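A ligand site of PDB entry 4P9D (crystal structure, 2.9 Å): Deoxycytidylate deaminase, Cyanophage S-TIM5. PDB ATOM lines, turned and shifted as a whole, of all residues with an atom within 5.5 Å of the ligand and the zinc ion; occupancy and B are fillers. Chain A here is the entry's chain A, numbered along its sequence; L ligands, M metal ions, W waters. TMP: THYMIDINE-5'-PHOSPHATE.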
ATOM      1  N   CYS A  25      -5.315 -27.932 -22.923  1.00  0.00           N
ATOM      2  CA  CYS A  25      -6.247 -26.888 -22.532  1.00  0.00           C
ATOM      3  C   CYS A  25      -6.411 -26.829 -21.011  1.00  0.00           C
ATOM      4  O   CYS A  25      -6.441 -27.857 -20.345  1.00  0.00           O
ATOM      5  CB  CYS A  25      -7.605 -27.094 -23.200  1.00  0.00           C
ATOM      6  SG  CYS A  25      -7.536 -27.226 -24.996  1.00  0.00           S
ATOM      7  N   ARG A  27      -8.763 -24.459 -19.538  1.00  0.00           N
ATOM      8  CA  ARG A  27     -10.170 -24.127 -19.286  1.00  0.00           C
ATOM      9  C   ARG A  27     -10.944 -25.377 -18.897  1.00  0.00           C
ATOM     10  O   ARG A  27     -11.675 -25.391 -17.902  1.00  0.00           O
ATOM     11  CB  ARG A  27     -10.793 -23.481 -20.517  1.00  0.00           C
ATOM     12  CG  ARG A  27     -10.452 -22.015 -20.721  1.00  0.00           C
ATOM     13  CD  ARG A  27     -11.358 -21.400 -21.781  1.00  0.00           C
ATOM     14  NE  ARG A  27     -12.767 -21.567 -21.466  1.00  0.00           N
ATOM     15  CZ  ARG A  27     -13.498 -20.682 -20.777  1.00  0.00           C
ATOM     16  NH1 ARG A  27     -12.937 -19.560 -20.337  1.00  0.00           N
ATOM     17  NH2 ARG A  27     -14.775 -20.925 -20.526  1.00  0.00           N
ATOM     18  N   MET A  28     -10.785 -26.419 -19.700  1.00  0.00           N
ATOM     19  CA  MET A  28     -11.488 -27.676 -19.489  1.00  0.00           C
ATOM     20  C   MET A  28     -10.838 -28.797 -20.285  1.00  0.00           C
ATOM     21  O   MET A  28     -10.550 -28.627 -21.470  1.00  0.00           O
ATOM     22  CB  MET A  28     -12.967 -27.528 -19.870  1.00  0.00           C
ATOM     23  CG  MET A  28     -13.884 -28.560 -19.244  1.00  0.00           C
ATOM     24  SD  MET A  28     -15.588 -28.356 -19.769  1.00  0.00           S
ATOM     25  CE  MET A  28     -16.442 -28.575 -18.218  1.00  0.00           C
ATOM     26  N   LYS A  29     -10.612 -29.940 -19.643  1.00  0.00           N
ATOM     27  CA  LYS A  29     -10.006 -31.080 -20.315  1.00  0.00           C
ATOM     28  C   LYS A  29     -11.025 -32.188 -20.539  1.00  0.00           C
ATOM     29  O   LYS A  29     -11.501 -32.819 -19.587  1.00  0.00           O
ATOM     30  CB  LYS A  29      -8.816 -31.603 -19.495  1.00  0.00           C
ATOM     31  CG  LYS A  29      -7.822 -30.529 -19.091  1.00  0.00           C
ATOM     32  CD  LYS A  29      -6.513 -31.156 -18.621  1.00  0.00           C
ATOM     33  CE  LYS A  29      -5.471 -30.094 -18.316  1.00  0.00           C
ATOM     34  NZ  LYS A  29      -4.077 -30.624 -18.393  1.00  0.00           N
ATOM     35  N   VAL A  30     -11.356 -32.431 -21.805  1.00  0.00           N
ATOM     36  CA  VAL A  30     -12.352 -33.420 -22.168  1.00  0.00           C
ATOM     37  C   VAL A  30     -11.741 -34.586 -22.940  1.00  0.00           C
ATOM     38  O   VAL A  30     -10.841 -34.385 -23.770  1.00  0.00           O
ATOM     39  CB  VAL A  30     -13.483 -32.799 -23.012  1.00  0.00           C
ATOM     40  CG1 VAL A  30     -14.694 -33.716 -23.059  1.00  0.00           C
ATOM     41  CG2 VAL A  30     -13.875 -31.455 -22.438  1.00  0.00           C
ATOM     42  N   ASN A  46      -9.691 -32.664 -26.498  1.00  0.00           N
ATOM     43  CA  ASN A  46      -9.741 -31.315 -27.044  1.00  0.00           C
ATOM     44  C   ASN A  46      -8.361 -30.710 -27.233  1.00  0.00           C
ATOM     45  O   ASN A  46      -7.455 -30.925 -26.416  1.00  0.00           O
ATOM     46  CB  ASN A  46     -10.593 -30.403 -26.157  1.00  0.00           C
ATOM     47  CG  ASN A  46     -10.100 -30.359 -24.729  1.00  0.00           C
ATOM     48  OD1 ASN A  46      -9.559 -31.331 -24.212  1.00  0.00           O
ATOM     49  ND2 ASN A  46     -10.280 -29.203 -24.088  1.00  0.00           N
ATOM     50  N   GLY A  47      -8.205 -29.941 -28.307  1.00  0.00           N
ATOM     51  CA  GLY A  47      -6.941 -29.291 -28.597  1.00  0.00           C
ATOM     52  C   GLY A  47      -6.919 -28.693 -29.991  1.00  0.00           C
ATOM     53  O   GLY A  47      -7.913 -28.747 -30.721  1.00  0.00           O
ATOM     54  N   CYS A  57      -4.274 -24.176 -25.982  1.00  0.00           N
ATOM     55  CA  CYS A  57      -5.632 -23.986 -26.479  1.00  0.00           C
ATOM     56  C   CYS A  57      -6.218 -22.622 -26.130  1.00  0.00           C
ATOM     57  O   CYS A  57      -7.275 -22.253 -26.638  1.00  0.00           O
ATOM     58  CB  CYS A  57      -6.538 -25.091 -25.943  1.00  0.00           C
ATOM     59  SG  CYS A  57      -5.746 -26.711 -25.795  1.00  0.00           S
ATOM     60  N   THR A  64     -10.991 -19.413 -25.314  1.00  0.00           N
ATOM     61  CA  THR A  64     -10.726 -20.574 -26.152  1.00  0.00           C
ATOM     62  C   THR A  64     -10.537 -20.187 -27.609  1.00  0.00           C
ATOM     63  O   THR A  64     -11.401 -19.553 -28.215  1.00  0.00           O
ATOM     64  CB  THR A  64     -11.867 -21.608 -26.040  1.00  0.00           C
ATOM     65  OG1 THR A  64     -11.689 -22.384 -24.848  1.00  0.00           O
ATOM     66  CG2 THR A  64     -11.864 -22.541 -27.233  1.00  0.00           C
ATOM     67  N   VAL A  68      -9.669 -24.652 -31.907  1.00  0.00           N
ATOM     68  CA  VAL A  68      -9.584 -25.914 -31.177  1.00  0.00           C
ATOM     69  C   VAL A  68     -10.721 -26.849 -31.545  1.00  0.00           C
ATOM     70  O   VAL A  68     -11.784 -26.416 -31.990  1.00  0.00           O
ATOM     71  CB  VAL A  68      -9.604 -25.706 -29.646  1.00  0.00           C
ATOM     72  CG1 VAL A  68      -8.589 -24.640 -29.233  1.00  0.00           C
ATOM     73  CG2 VAL A  68     -11.001 -25.337 -29.161  1.00  0.00           C
ATOM     74  N   LEU A  69     -10.480 -28.140 -31.379  1.00  0.00           N
ATOM     75  CA  LEU A  69     -11.469 -29.169 -31.661  1.00  0.00           C
ATOM     76  C   LEU A  69     -12.020 -29.713 -30.362  1.00  0.00           C
ATOM     77  O   LEU A  69     -11.287 -29.851 -29.378  1.00  0.00           O
ATOM     78  CB  LEU A  69     -10.864 -30.288 -32.502  1.00  0.00           C
ATOM     79  CG  LEU A  69     -10.376 -29.918 -33.905  1.00  0.00           C
ATOM     80  CD1 LEU A  69      -9.095 -30.672 -34.231  1.00  0.00           C
ATOM     81  CD2 LEU A  69     -11.444 -30.219 -34.934  1.00  0.00           C
ATOM     82  N   HIS A  70     -13.309 -30.030 -30.338  1.00  0.00           N
ATOM     83  CA  HIS A  70     -13.891 -30.708 -29.188  1.00  0.00           C
ATOM     84  C   HIS A  70     -13.397 -32.153 -29.179  1.00  0.00           C
ATOM     85  O   HIS A  70     -13.043 -32.706 -30.221  1.00  0.00           O
ATOM     86  CB  HIS A  70     -15.410 -30.654 -29.219  1.00  0.00           C
ATOM     87  CG  HIS A  70     -15.976 -29.313 -28.852  1.00  0.00           C
ATOM     88  ND1 HIS A  70     -17.329 -29.072 -28.752  1.00  0.00           N
ATOM     89  CD2 HIS A  70     -15.364 -28.144 -28.546  1.00  0.00           C
ATOM     90  CE1 HIS A  70     -17.526 -27.815 -28.416  1.00  0.00           C
ATOM     91  NE2 HIS A  70     -16.354 -27.231 -28.277  1.00  0.00           N
ATOM     92  N   ALA A  71     -13.383 -32.759 -27.991  1.00  0.00           N
ATOM     93  CA  ALA A  71     -12.967 -34.150 -27.848  1.00  0.00           C
ATOM     94  C   ALA A  71     -13.839 -35.057 -28.712  1.00  0.00           C
ATOM     95  O   ALA A  71     -13.361 -36.025 -29.303  1.00  0.00           O
ATOM     96  CB  ALA A  71     -13.039 -34.575 -26.392  1.00  0.00           C
ATOM     97  N   GLU A  72     -15.121 -34.724 -28.781  1.00  0.00           N
ATOM     98  CA  GLU A  72     -16.085 -35.481 -29.565  1.00  0.00           C
ATOM     99  C   GLU A  72     -15.836 -35.284 -31.058  1.00  0.00           C
ATOM    100  O   GLU A  72     -16.056 -36.179 -31.857  1.00  0.00           O
ATOM    101  CB  GLU A  72     -17.510 -35.072 -29.207  1.00  0.00           C
ATOM    102  CG  GLU A  72     -17.915 -35.345 -27.748  1.00  0.00           C
ATOM    103  CD  GLU A  72     -17.233 -34.415 -26.765  1.00  0.00           C
ATOM    104  OE1 GLU A  72     -16.962 -33.250 -27.130  1.00  0.00           O
ATOM    105  OE2 GLU A  72     -16.966 -34.848 -25.622  1.00  0.00           O
ATOM    106  N   GLN A  73     -15.373 -34.087 -31.416  1.00  0.00           N
ATOM    107  CA  GLN A  73     -15.062 -33.770 -32.815  1.00  0.00           C
ATOM    108  C   GLN A  73     -13.868 -34.583 -33.302  1.00  0.00           C
ATOM    109  O   GLN A  73     -13.915 -35.169 -34.387  1.00  0.00           O
ATOM    110  CB  GLN A  73     -14.789 -32.277 -32.977  1.00  0.00           C
ATOM    111  CG  GLN A  73     -15.988 -31.465 -33.446  1.00  0.00           C
ATOM    112  CD  GLN A  73     -15.679 -29.984 -33.514  1.00  0.00           C
ATOM    113  OE1 GLN A  73     -14.974 -29.445 -32.668  1.00  0.00           O
ATOM    114  NE2 GLN A  73     -16.220 -29.314 -34.530  1.00  0.00           N
ATOM    115  N   SER A  96     -20.474 -34.198 -20.852  1.00  0.00           N
ATOM    116  CA  SER A  96     -21.576 -34.249 -21.800  1.00  0.00           C
ATOM    117  C   SER A  96     -21.305 -33.344 -23.002  1.00  0.00           C
ATOM    118  O   SER A  96     -20.907 -32.184 -22.836  1.00  0.00           O
ATOM    119  CB  SER A  96     -22.880 -33.846 -21.116  1.00  0.00           C
ATOM    120  OG  SER A  96     -22.840 -32.498 -20.684  1.00  0.00           O
ATOM    121  N   PRO A  97     -21.514 -33.869 -24.218  1.00  0.00           N
ATOM    122  CA  PRO A  97     -21.169 -33.183 -25.458  1.00  0.00           C
ATOM    123  C   PRO A  97     -22.070 -31.985 -25.780  1.00  0.00           C
ATOM    124  O   PRO A  97     -23.195 -31.905 -25.293  1.00  0.00           O
ATOM    125  CB  PRO A  97     -21.327 -34.272 -26.514  1.00  0.00           C
ATOM    126  CG  PRO A  97     -22.367 -35.173 -25.957  1.00  0.00           C
ATOM    127  CD  PRO A  97     -22.121 -35.191 -24.477  1.00  0.00           C
ATOM    128  N   CYS A  98     -21.552 -31.066 -26.594  1.00  0.00           N
ATOM    129  CA  CYS A  98     -22.277 -29.869 -27.013  1.00  0.00           C
ATOM    130  C   CYS A  98     -23.304 -30.240 -28.089  1.00  0.00           C
ATOM    131  O   CYS A  98     -23.213 -31.322 -28.678  1.00  0.00           O
ATOM    132  CB  CYS A  98     -21.302 -28.805 -27.525  1.00  0.00           C
ATOM    133  SG  CYS A  98     -20.612 -29.155 -29.159  1.00  0.00           S
ATOM    134  N   ASP A 100     -23.725 -29.247 -31.208  1.00  0.00           N
ATOM    135  CA  ASP A 100     -23.192 -29.448 -32.554  1.00  0.00           C
ATOM    136  C   ASP A 100     -22.624 -30.848 -32.738  1.00  0.00           C
ATOM    137  O   ASP A 100     -22.939 -31.533 -33.697  1.00  0.00           O
ATOM    138  CB  ASP A 100     -22.125 -28.403 -32.877  1.00  0.00           C
ATOM    139  CG  ASP A 100     -21.707 -28.431 -34.334  1.00  0.00           C
ATOM    140  OD1 ASP A 100     -22.602 -28.380 -35.213  1.00  0.00           O
ATOM    141  OD2 ASP A 100     -20.498 -28.511 -34.602  1.00  0.00           O
ATOM    142  N   CYS A 101     -21.777 -31.266 -31.802  1.00  0.00           N
ATOM    143  CA  CYS A 101     -21.224 -32.613 -31.818  1.00  0.00           C
ATOM    144  C   CYS A 101     -22.336 -33.642 -31.662  1.00  0.00           C
ATOM    145  O   CYS A 101     -22.290 -34.715 -32.260  1.00  0.00           O
ATOM    146  CB  CYS A 101     -20.175 -32.789 -30.712  1.00  0.00           C
ATOM    147  SG  CYS A 101     -18.769 -31.646 -30.807  1.00  0.00           S
ATOM    148  N   TYR A 119     -21.922 -31.103 -18.107  1.00  0.00           N
ATOM    149  CA  TYR A 119     -21.475 -29.756 -18.461  1.00  0.00           C
ATOM    150  C   TYR A 119     -22.437 -28.669 -17.976  1.00  0.00           C
ATOM    151  O   TYR A 119     -23.586 -28.945 -17.639  1.00  0.00           O
ATOM    152  CB  TYR A 119     -21.298 -29.653 -19.981  1.00  0.00           C
ATOM    153  CG  TYR A 119     -20.660 -28.359 -20.461  1.00  0.00           C
ATOM    154  CD1 TYR A 119     -19.440 -27.925 -19.950  1.00  0.00           C
ATOM    155  CD2 TYR A 119     -21.275 -27.576 -21.426  1.00  0.00           C
ATOM    156  CE1 TYR A 119     -18.861 -26.752 -20.376  1.00  0.00           C
ATOM    157  CE2 TYR A 119     -20.700 -26.401 -21.861  1.00  0.00           C
ATOM    158  CZ  TYR A 119     -19.497 -25.991 -21.334  1.00  0.00           C
ATOM    159  OH  TYR A 119     -18.927 -24.815 -21.777  1.00  0.00           O
ATOM    160  N   ARG A 120     -21.931 -27.431 -17.911  1.00  0.00           N
ATOM    161  CA  ARG A 120     -22.725 -26.237 -17.634  1.00  0.00           C
ATOM    162  C   ARG A 120     -24.055 -26.288 -18.355  1.00  0.00           C
ATOM    163  O   ARG A 120     -25.099 -26.549 -17.760  1.00  0.00           O
ATOM    164  CB  ARG A 120     -21.972 -24.987 -18.069  1.00  0.00           C
ATOM    165  CG  ARG A 120     -20.799 -24.585 -17.204  1.00  0.00           C
ATOM    166  CD  ARG A 120     -20.143 -23.352 -17.799  1.00  0.00           C
ATOM    167  NE  ARG A 120     -20.589 -23.119 -19.174  1.00  0.00           N
ATOM    168  CZ  ARG A 120     -21.035 -21.948 -19.622  1.00  0.00           C
ATOM    169  NH1 ARG A 120     -21.081 -20.903 -18.810  1.00  0.00           N
ATOM    170  NH2 ARG A 120     -21.421 -21.819 -20.876  1.00  0.00           N
HETATM  171  P   TMP L   1     -15.401 -23.358 -23.595  1.00  0.00           P
HETATM  172  O1P TMP L   1     -14.287 -22.420 -23.746  1.00  0.00           O
HETATM  173  O2P TMP L   1     -16.259 -23.485 -24.795  1.00  0.00           O
HETATM  174  O3P TMP L   1     -16.143 -23.281 -22.322  1.00  0.00           O
HETATM  175  O5' TMP L   1     -14.709 -24.781 -23.551  1.00  0.00           O
HETATM  176  C5' TMP L   1     -13.396 -24.907 -22.971  1.00  0.00           C
HETATM  177  C4' TMP L   1     -12.660 -26.171 -23.438  1.00  0.00           C
HETATM  178  O4' TMP L   1     -13.577 -27.301 -23.398  1.00  0.00           O
HETATM  179  C3' TMP L   1     -12.236 -26.073 -24.896  1.00  0.00           C
HETATM  180  O3' TMP L   1     -11.154 -26.984 -25.146  1.00  0.00           O
HETATM  181  C2' TMP L   1     -13.451 -26.632 -25.573  1.00  0.00           C
HETATM  182  C1' TMP L   1     -13.543 -27.869 -24.720  1.00  0.00           C
HETATM  183  N1  TMP L   1     -14.801 -28.618 -24.949  1.00  0.00           N
HETATM  184  C2  TMP L   1     -14.779 -29.877 -25.409  1.00  0.00           C
HETATM  185  O2  TMP L   1     -13.706 -30.428 -25.663  1.00  0.00           O
HETATM  186  N3  TMP L   1     -15.970 -30.576 -25.620  1.00  0.00           N
HETATM  187  C4  TMP L   1     -17.201 -29.963 -25.349  1.00  0.00           C
HETATM  188  O4  TMP L   1     -18.256 -30.578 -25.535  1.00  0.00           O
HETATM  189  C5  TMP L   1     -17.215 -28.662 -24.873  1.00  0.00           C
HETATM  190  C5M TMP L   1     -18.423 -28.035 -24.589  1.00  0.00           C
HETATM  191  C6  TMP L   1     -16.015 -27.989 -24.674  1.00  0.00           C
HETATM  192 ZN    ZN M   1     -18.808 -30.455 -28.861  1.00  0.00          ZN
HETATM  193  O   HOH W   1     -18.829 -31.864 -27.330  1.00  0.00           O
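OE1 of Gln 73 lies within hydrogen-bond range of N of His 70.
The side-chain sulfur (SG) of Cys 98 sits close to the backbone NH (N) of Asp 100 (3.7 Å).
OD1 of Asn 46 lies within hydrogen-bond range of N of Val 30.
ND2 of Asn 46 lies within hydrogen-bond range of O of Met 28 (2.7 Å).
The side-chain amide nitrogen (ND2) of Asn 46 sits at hydrogen-bond distance from the side-chain sulfur (SG) of Cys 25 (3.5 Å).
The backbone NH of Tyr 119 lies within hydrogen-bond range of the side-chain hydroxyl of Ser 96 (3.1 Å).
SG of Cys 57 is disulfide-bonded to SG of Cys 25, at 2.0 Å.
ND1 of His 70 binds the zinc ion, at 2.0 Å.
The zinc ion is bound by water W1 (2.1 Å).
The zinc ion is bound by SG of Cys 98 (2.2 Å).
The zinc ion is bound by SG of Cys 101, 2.3 Å away.
The zinc ion has four donor atoms within binding distance.
Merely in contact with the ligand: Val 30 (3.4 Å), Met 28 (3.6 Å) and Pro 97 (3.9 Å).
Hydrophobic or aromatic side chains that line the ligand: Met 28, Val 30, His 70 and Tyr 119.
Of the 22 residues printed, 12 come within 4 Å of the ligand.
O4 of the ligand lies within hydrogen-bond range of N of Cys 98, 3.5 Å away.
ND2 of Asn 46 sits at hydrogen-bond distance from O3' of the ligand (2.6 Å).
An oxygen (O1P) of the ligand is in hydrogen-bond range of the side-chain hydroxyl (OG1) of Thr 64, at 2.8 Å.
NE of Arg 27 lies within salt-bridge range of O1P of the ligand, at 2.9 Å.
O3P of the ligand lies within hydrogen-bond range of OH of Tyr 119, 3.2 Å away.
The side-chain carboxylate of Glu 72 sits at hydrogen-bond distance from a nitrogen (N3) of the ligand (3.2 Å).
The backbone NH of Ala 71 lies within hydrogen-bond range of an oxygen (O2) of the ligand.
SG of Cys 25 sits at hydrogen-bond distance from O3' of the ligand.
Merely in contact with the zinc ion: Glu 72 (3.8 Å).
Within 4 Å of the zinc ion: His 70, Glu 72, Cys 98 and Cys 101.
The nearest printed residue that does not touch the zinc ion is Pro 97 (4.7 Å).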
